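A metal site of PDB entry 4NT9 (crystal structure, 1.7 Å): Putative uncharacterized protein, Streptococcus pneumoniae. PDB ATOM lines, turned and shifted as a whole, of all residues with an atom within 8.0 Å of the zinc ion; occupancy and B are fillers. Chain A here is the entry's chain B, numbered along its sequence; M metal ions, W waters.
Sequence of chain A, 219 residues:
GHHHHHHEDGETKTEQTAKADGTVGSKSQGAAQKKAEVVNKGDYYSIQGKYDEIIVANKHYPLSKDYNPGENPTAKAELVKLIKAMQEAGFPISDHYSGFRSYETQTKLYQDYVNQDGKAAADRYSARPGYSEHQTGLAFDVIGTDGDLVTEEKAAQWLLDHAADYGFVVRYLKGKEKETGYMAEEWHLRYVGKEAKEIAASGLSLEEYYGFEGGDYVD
The backbone NH (N) of Asp 141 is in hydrogen-bond range of the backbone carbonyl oxygen (O) of Ser 98.
O of His 188 sits at hydrogen-bond distance from N of Arg 171 (3.3 Å).
A ring nitrogen (ND1) of His 134 sits at hydrogen-bond distance from the backbone carbonyl oxygen of Ala 139, 3.4 Å away.
The backbone NH (N) of His 134 lies close to the side-chain hydroxyl (OG) of Ser 132 (3.1 Å).
The backbone carbonyl oxygen (O) of Tyr 172 lies within hydrogen-bond range of the backbone NH (N) of Glu 185 (3.0 Å).
A ring nitrogen (NE2) of His 188 lies within hydrogen-bond range of the side-chain carboxylate of Glu 133 (2.9 Å).
OD1 of Asp 141 lies close to NE1 of Trp 187.
The guanidinium group (NH2) of Arg 101 is in salt-bridge range of the side-chain carboxylate (OD2) of Asp 141.
The nearest printed residue that does not touch the zinc ion is Trp 187 (4.2 Å).
The zinc ion is bound by ND1 of His 188 (2.0 Å), water W1 (2.0 Å), NE2 of His 134 (2.1 Å), OD1 of Asp 141 (2.1 Å), water W2 (2.1 Å) and OE1 of Glu 185 (2.2 Å).
Water W1 lies within hydrogen-bond range of OD2 of Asp 141 (2.8 Å) and NH1 of Arg 101 (3.1 Å).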
ATOM      1  N   SER A  98     -24.551  27.208  26.192  1.00  0.00           N
ATOM      2  CA  SER A  98     -25.287  26.235  26.996  1.00  0.00           C
ATOM      3  C   SER A  98     -24.557  24.888  26.902  1.00  0.00           C
ATOM      4  O   SER A  98     -24.594  24.234  25.826  1.00  0.00           O
ATOM      5  CB  SER A  98     -26.725  26.047  26.513  1.00  0.00           C
ATOM      6  OG  SER A  98     -27.400  25.071  27.315  1.00  0.00           O
ATOM      7  N   GLY A  99     -23.921  24.472  28.015  1.00  0.00           N
ATOM      8  CA  GLY A  99     -23.017  23.307  28.034  1.00  0.00           C
ATOM      9  C   GLY A  99     -23.733  22.201  28.818  1.00  0.00           C
ATOM     10  O   GLY A  99     -24.739  21.664  28.343  1.00  0.00           O
ATOM     11  N   ARG A 101     -26.267  20.318  31.084  1.00  0.00           N
ATOM     12  CA  ARG A 101     -27.604  20.504  31.622  1.00  0.00           C
ATOM     13  C   ARG A 101     -27.940  19.209  32.328  1.00  0.00           C
ATOM     14  O   ARG A 101     -28.057  18.179  31.694  1.00  0.00           O
ATOM     15  CB  ARG A 101     -28.664  20.826  30.557  1.00  0.00           C
ATOM     16  CG  ARG A 101     -28.349  22.077  29.711  1.00  0.00           C
ATOM     17  CD  ARG A 101     -29.550  22.611  28.949  1.00  0.00           C
ATOM     18  NE  ARG A 101     -29.999  21.863  27.764  1.00  0.00           N
ATOM     19  CZ  ARG A 101     -29.718  22.208  26.510  1.00  0.00           C
ATOM     20  NH1 ARG A 101     -30.233  21.515  25.492  1.00  0.00           N
ATOM     21  NH2 ARG A 101     -28.907  23.225  26.255  1.00  0.00           N
ATOM     22  N   GLN A 106     -32.785  19.810  32.509  1.00  0.00           N
ATOM     23  CA  GLN A 106     -33.421  19.429  31.256  1.00  0.00           C
ATOM     24  C   GLN A 106     -34.902  19.216  31.470  1.00  0.00           C
ATOM     25  O   GLN A 106     -35.701  19.518  30.588  1.00  0.00           O
ATOM     26  CB  GLN A 106     -32.786  18.142  30.697  1.00  0.00           C
ATOM     27  CG  GLN A 106     -33.240  17.810  29.284  1.00  0.00           C
ATOM     28  CD  GLN A 106     -32.713  18.815  28.244  1.00  0.00           C
ATOM     29  OE1 GLN A 106     -31.629  19.391  28.411  1.00  0.00           O
ATOM     30  NE2 GLN A 106     -33.462  18.998  27.183  1.00  0.00           N
ATOM     31  N   TYR A 125     -38.422  20.164  18.963  1.00  0.00           N
ATOM     32  CA  TYR A 125     -37.196  20.948  19.091  1.00  0.00           C
ATOM     33  C   TYR A 125     -36.439  20.832  20.405  1.00  0.00           C
ATOM     34  O   TYR A 125     -35.256  21.247  20.471  1.00  0.00           O
ATOM     35  CB  TYR A 125     -37.424  22.424  18.724  1.00  0.00           C
ATOM     36  CG  TYR A 125     -38.223  23.230  19.711  1.00  0.00           C
ATOM     37  CD1 TYR A 125     -37.674  23.624  20.934  1.00  0.00           C
ATOM     38  CD2 TYR A 125     -39.509  23.648  19.409  1.00  0.00           C
ATOM     39  CE1 TYR A 125     -38.395  24.365  21.844  1.00  0.00           C
ATOM     40  CE2 TYR A 125     -40.239  24.402  20.313  1.00  0.00           C
ATOM     41  CZ  TYR A 125     -39.676  24.757  21.529  1.00  0.00           C
ATOM     42  OH  TYR A 125     -40.395  25.503  22.431  1.00  0.00           O
ATOM     43  N   SER A 132     -31.146  14.195  26.276  1.00  0.00           N
ATOM     44  CA  SER A 132     -30.349  15.297  25.708  1.00  0.00           C
ATOM     45  C   SER A 132     -28.868  15.013  25.863  1.00  0.00           C
ATOM     46  O   SER A 132     -28.417  14.700  26.964  1.00  0.00           O
ATOM     47  CB  SER A 132     -30.586  16.583  26.472  1.00  0.00           C
ATOM     48  OG  SER A 132     -29.752  17.619  25.889  1.00  0.00           O
ATOM     49  N   GLU A 133     -28.094  15.155  24.794  1.00  0.00           N
ATOM     50  CA  GLU A 133     -26.642  15.009  24.912  1.00  0.00           C
ATOM     51  C   GLU A 133     -26.012  16.029  25.893  1.00  0.00           C
ATOM     52  O   GLU A 133     -24.889  15.863  26.343  1.00  0.00           O
ATOM     53  CB  GLU A 133     -26.027  15.136  23.511  1.00  0.00           C
ATOM     54  CG  GLU A 133     -24.649  14.575  23.424  1.00  0.00           C
ATOM     55  CD  GLU A 133     -24.075  14.682  22.029  1.00  0.00           C
ATOM     56  OE1 GLU A 133     -23.586  13.648  21.485  1.00  0.00           O
ATOM     57  OE2 GLU A 133     -24.074  15.820  21.457  1.00  0.00           O
ATOM     58  N   HIS A 134     -26.715  17.117  26.222  1.00  0.00           N
ATOM     59  CA  HIS A 134     -26.166  18.102  27.159  1.00  0.00           C
ATOM     60  C   HIS A 134     -25.986  17.527  28.555  1.00  0.00           C
ATOM     61  O   HIS A 134     -25.210  18.066  29.368  1.00  0.00           O
ATOM     62  CB  HIS A 134     -27.054  19.343  27.194  1.00  0.00           C
ATOM     63  CG  HIS A 134     -26.962  20.133  25.921  1.00  0.00           C
ATOM     64  ND1 HIS A 134     -25.996  21.111  25.718  1.00  0.00           N
ATOM     65  CD2 HIS A 134     -27.650  20.032  24.769  1.00  0.00           C
ATOM     66  CE1 HIS A 134     -26.138  21.612  24.506  1.00  0.00           C
ATOM     67  NE2 HIS A 134     -27.145  20.969  23.906  1.00  0.00           N
ATOM     68  N   ALA A 139     -21.409  18.287  25.478  1.00  0.00           N
ATOM     69  CA  ALA A 139     -22.102  18.992  24.379  1.00  0.00           C
ATOM     70  C   ALA A 139     -22.364  20.466  24.712  1.00  0.00           C
ATOM     71  O   ALA A 139     -22.618  20.821  25.878  1.00  0.00           O
ATOM     72  CB  ALA A 139     -23.439  18.316  24.116  1.00  0.00           C
ATOM     73  N   PHE A 140     -22.227  21.342  23.708  1.00  0.00           N
ATOM     74  CA  PHE A 140     -22.270  22.781  23.969  1.00  0.00           C
ATOM     75  C   PHE A 140     -23.019  23.479  22.846  1.00  0.00           C
ATOM     76  O   PHE A 140     -22.680  23.294  21.679  1.00  0.00           O
ATOM     77  CB  PHE A 140     -20.827  23.337  24.028  1.00  0.00           C
ATOM     78  CG  PHE A 140     -19.969  22.667  25.060  1.00  0.00           C
ATOM     79  CD1 PHE A 140     -19.313  21.465  24.789  1.00  0.00           C
ATOM     80  CD2 PHE A 140     -19.882  23.201  26.321  1.00  0.00           C
ATOM     81  CE1 PHE A 140     -18.552  20.817  25.792  1.00  0.00           C
ATOM     82  CE2 PHE A 140     -19.110  22.585  27.309  1.00  0.00           C
ATOM     83  CZ  PHE A 140     -18.473  21.383  27.034  1.00  0.00           C
ATOM     84  N   ASP A 141     -24.021  24.276  23.200  1.00  0.00           N
ATOM     85  CA  ASP A 141     -24.689  25.126  22.203  1.00  0.00           C
ATOM     86  C   ASP A 141     -24.004  26.481  22.204  1.00  0.00           C
ATOM     87  O   ASP A 141     -23.892  27.134  23.258  1.00  0.00           O
ATOM     88  CB  ASP A 141     -26.168  25.405  22.560  1.00  0.00           C
ATOM     89  CG  ASP A 141     -27.030  24.167  22.657  1.00  0.00           C
ATOM     90  OD1 ASP A 141     -26.819  23.134  21.964  1.00  0.00           O
ATOM     91  OD2 ASP A 141     -28.022  24.239  23.435  1.00  0.00           O
ATOM     92  N   VAL A 142     -23.569  26.909  21.031  1.00  0.00           N
ATOM     93  CA  VAL A 142     -22.895  28.174  20.847  1.00  0.00           C
ATOM     94  C   VAL A 142     -23.956  29.269  20.605  1.00  0.00           C
ATOM     95  O   VAL A 142     -24.960  29.051  19.897  1.00  0.00           O
ATOM     96  CB  VAL A 142     -21.902  28.099  19.646  1.00  0.00           C
ATOM     97  CG1 VAL A 142     -21.219  29.414  19.409  1.00  0.00           C
ATOM     98  CG2 VAL A 142     -20.814  27.054  19.953  1.00  0.00           C
ATOM     99  N   LEU A 149     -29.152  31.427  19.676  1.00  0.00           N
ATOM    100  CA  LEU A 149     -28.297  30.333  19.199  1.00  0.00           C
ATOM    101  C   LEU A 149     -27.733  30.651  17.808  1.00  0.00           C
ATOM    102  O   LEU A 149     -28.421  31.248  16.973  1.00  0.00           O
ATOM    103  CB  LEU A 149     -29.102  29.058  19.116  1.00  0.00           C
ATOM    104  CG  LEU A 149     -29.604  28.676  20.518  1.00  0.00           C
ATOM    105  CD1 LEU A 149     -30.785  27.742  20.455  1.00  0.00           C
ATOM    106  CD2 LEU A 149     -28.442  28.055  21.285  1.00  0.00           C
ATOM    107  N   ARG A 171     -22.966  17.975  15.780  1.00  0.00           N
ATOM    108  CA  ARG A 171     -23.601  16.707  16.026  1.00  0.00           C
ATOM    109  C   ARG A 171     -24.831  16.448  15.177  1.00  0.00           C
ATOM    110  O   ARG A 171     -25.048  15.333  14.709  1.00  0.00           O
ATOM    111  CB  ARG A 171     -24.042  16.677  17.507  1.00  0.00           C
ATOM    112  CG  ARG A 171     -24.556  15.347  17.981  1.00  0.00           C
ATOM    113  CD  ARG A 171     -23.436  14.304  18.067  1.00  0.00           C
ATOM    114  NE  ARG A 171     -23.909  13.078  18.728  1.00  0.00           N
ATOM    115  CZ  ARG A 171     -24.541  12.066  18.116  1.00  0.00           C
ATOM    116  NH1 ARG A 171     -24.782  12.120  16.780  1.00  0.00           N
ATOM    117  NH2 ARG A 171     -24.912  11.001  18.844  1.00  0.00           N
ATOM    118  N   TYR A 172     -25.626  17.483  14.996  1.00  0.00           N
ATOM    119  CA  TYR A 172     -26.952  17.332  14.403  1.00  0.00           C
ATOM    120  C   TYR A 172     -27.041  18.135  13.117  1.00  0.00           C
ATOM    121  O   TYR A 172     -27.332  19.322  13.136  1.00  0.00           O
ATOM    122  CB  TYR A 172     -28.004  17.866  15.387  1.00  0.00           C
ATOM    123  CG  TYR A 172     -28.009  17.125  16.724  1.00  0.00           C
ATOM    124  CD1 TYR A 172     -28.064  15.744  16.795  1.00  0.00           C
ATOM    125  CD2 TYR A 172     -27.882  17.832  17.899  1.00  0.00           C
ATOM    126  CE1 TYR A 172     -28.051  15.094  18.021  1.00  0.00           C
ATOM    127  CE2 TYR A 172     -27.893  17.181  19.144  1.00  0.00           C
ATOM    128  CZ  TYR A 172     -27.973  15.826  19.178  1.00  0.00           C
ATOM    129  OH  TYR A 172     -27.957  15.171  20.392  1.00  0.00           O
ATOM    130  N   TYR A 182     -32.654  13.819  15.925  1.00  0.00           N
ATOM    131  CA  TYR A 182     -32.831  15.194  16.415  1.00  0.00           C
ATOM    132  C   TYR A 182     -32.930  16.185  15.293  1.00  0.00           C
ATOM    133  O   TYR A 182     -32.308  16.044  14.233  1.00  0.00           O
ATOM    134  CB  TYR A 182     -31.648  15.612  17.315  1.00  0.00           C
ATOM    135  CG  TYR A 182     -31.534  14.788  18.582  1.00  0.00           C
ATOM    136  CD1 TYR A 182     -31.069  13.470  18.537  1.00  0.00           C
ATOM    137  CD2 TYR A 182     -31.880  15.322  19.814  1.00  0.00           C
ATOM    138  CE1 TYR A 182     -30.956  12.726  19.687  1.00  0.00           C
ATOM    139  CE2 TYR A 182     -31.759  14.569  20.983  1.00  0.00           C
ATOM    140  CZ  TYR A 182     -31.299  13.269  20.901  1.00  0.00           C
ATOM    141  OH  TYR A 182     -31.203  12.502  22.047  1.00  0.00           O
ATOM    142  N   MET A 183     -33.718  17.233  15.542  1.00  0.00           N
ATOM    143  CA  MET A 183     -33.772  18.365  14.626  1.00  0.00           C
ATOM    144  C   MET A 183     -32.370  18.937  14.527  1.00  0.00           C
ATOM    145  O   MET A 183     -31.642  19.004  15.532  1.00  0.00           O
ATOM    146  CB  MET A 183     -34.685  19.438  15.197  1.00  0.00           C
ATOM    147  CG  MET A 183     -34.866  20.613  14.294  1.00  0.00           C
ATOM    148  SD  MET A 183     -36.431  21.480  14.644  1.00  0.00           S
ATOM    149  CE  MET A 183     -35.899  22.670  15.775  1.00  0.00           C
ATOM    150  N   GLU A 185     -29.154  21.196  14.626  1.00  0.00           N
ATOM    151  CA  GLU A 185     -28.703  22.307  15.463  1.00  0.00           C
ATOM    152  C   GLU A 185     -27.414  22.835  14.854  1.00  0.00           C
ATOM    153  O   GLU A 185     -26.365  22.200  15.003  1.00  0.00           O
ATOM    154  CB  GLU A 185     -28.475  21.814  16.911  1.00  0.00           C
ATOM    155  CG  GLU A 185     -29.749  21.412  17.725  1.00  0.00           C
ATOM    156  CD  GLU A 185     -29.450  20.967  19.164  1.00  0.00           C
ATOM    157  OE1 GLU A 185     -28.642  21.606  19.897  1.00  0.00           O
ATOM    158  OE2 GLU A 185     -30.013  19.925  19.563  1.00  0.00           O
ATOM    159  N   TRP A 187     -25.635  25.065  15.898  1.00  0.00           N
ATOM    160  CA  TRP A 187     -24.894  25.669  16.978  1.00  0.00           C
ATOM    161  C   TRP A 187     -24.380  24.630  17.975  1.00  0.00           C
ATOM    162  O   TRP A 187     -23.738  24.997  18.938  1.00  0.00           O
ATOM    163  CB  TRP A 187     -25.844  26.544  17.781  1.00  0.00           C
ATOM    164  CG  TRP A 187     -27.104  25.816  18.234  1.00  0.00           C
ATOM    165  CD1 TRP A 187     -27.257  24.994  19.354  1.00  0.00           C
ATOM    166  CD2 TRP A 187     -28.383  25.828  17.575  1.00  0.00           C
ATOM    167  NE1 TRP A 187     -28.564  24.533  19.413  1.00  0.00           N
ATOM    168  CE2 TRP A 187     -29.262  25.036  18.334  1.00  0.00           C
ATOM    169  CE3 TRP A 187     -28.866  26.448  16.411  1.00  0.00           C
ATOM    170  CZ2 TRP A 187     -30.599  24.839  17.966  1.00  0.00           C
ATOM    171  CZ3 TRP A 187     -30.186  26.256  16.060  1.00  0.00           C
ATOM    172  CH2 TRP A 187     -31.034  25.457  16.821  1.00  0.00           C
ATOM    173  N   HIS A 188     -24.678  23.350  17.749  1.00  0.00           N
ATOM    174  CA  HIS A 188     -24.447  22.343  18.828  1.00  0.00           C
ATOM    175  C   HIS A 188     -23.216  21.488  18.563  1.00  0.00           C
ATOM    176  O   HIS A 188     -23.128  20.791  17.544  1.00  0.00           O
ATOM    177  CB  HIS A 188     -25.717  21.472  19.000  1.00  0.00           C
ATOM    178  CG  HIS A 188     -25.554  20.323  19.936  1.00  0.00           C
ATOM    179  ND1 HIS A 188     -26.314  20.163  21.090  1.00  0.00           N
ATOM    180  CD2 HIS A 188     -24.733  19.249  19.886  1.00  0.00           C
ATOM    181  CE1 HIS A 188     -25.971  19.031  21.679  1.00  0.00           C
ATOM    182  NE2 HIS A 188     -24.985  18.480  20.982  1.00  0.00           N
ATOM    183  N   LEU A 189     -22.255  21.579  19.472  1.00  0.00           N
ATOM    184  CA  LEU A 189     -20.977  20.888  19.300  1.00  0.00           C
ATOM    185  C   LEU A 189     -20.853  19.768  20.324  1.00  0.00           C
ATOM    186  O   LEU A 189     -21.131  19.988  21.485  1.00  0.00           O
ATOM    187  CB  LEU A 189     -19.881  21.885  19.574  1.00  0.00           C
ATOM    188  CG  LEU A 189     -19.763  23.024  18.555  1.00  0.00           C
ATOM    189  CD1 LEU A 189     -18.657  23.958  19.004  1.00  0.00           C
ATOM    190  CD2 LEU A 189     -19.424  22.459  17.158  1.00  0.00           C
HETATM  191 ZN    ZN M   1     -27.807  21.255  21.912  1.00  0.00          ZN
HETATM  192  O   HOH W   1     -29.532  22.096  22.563  1.00  0.00           O
HETATM  193  O   HOH W   2     -28.918  19.442  21.896  1.00  0.00           O
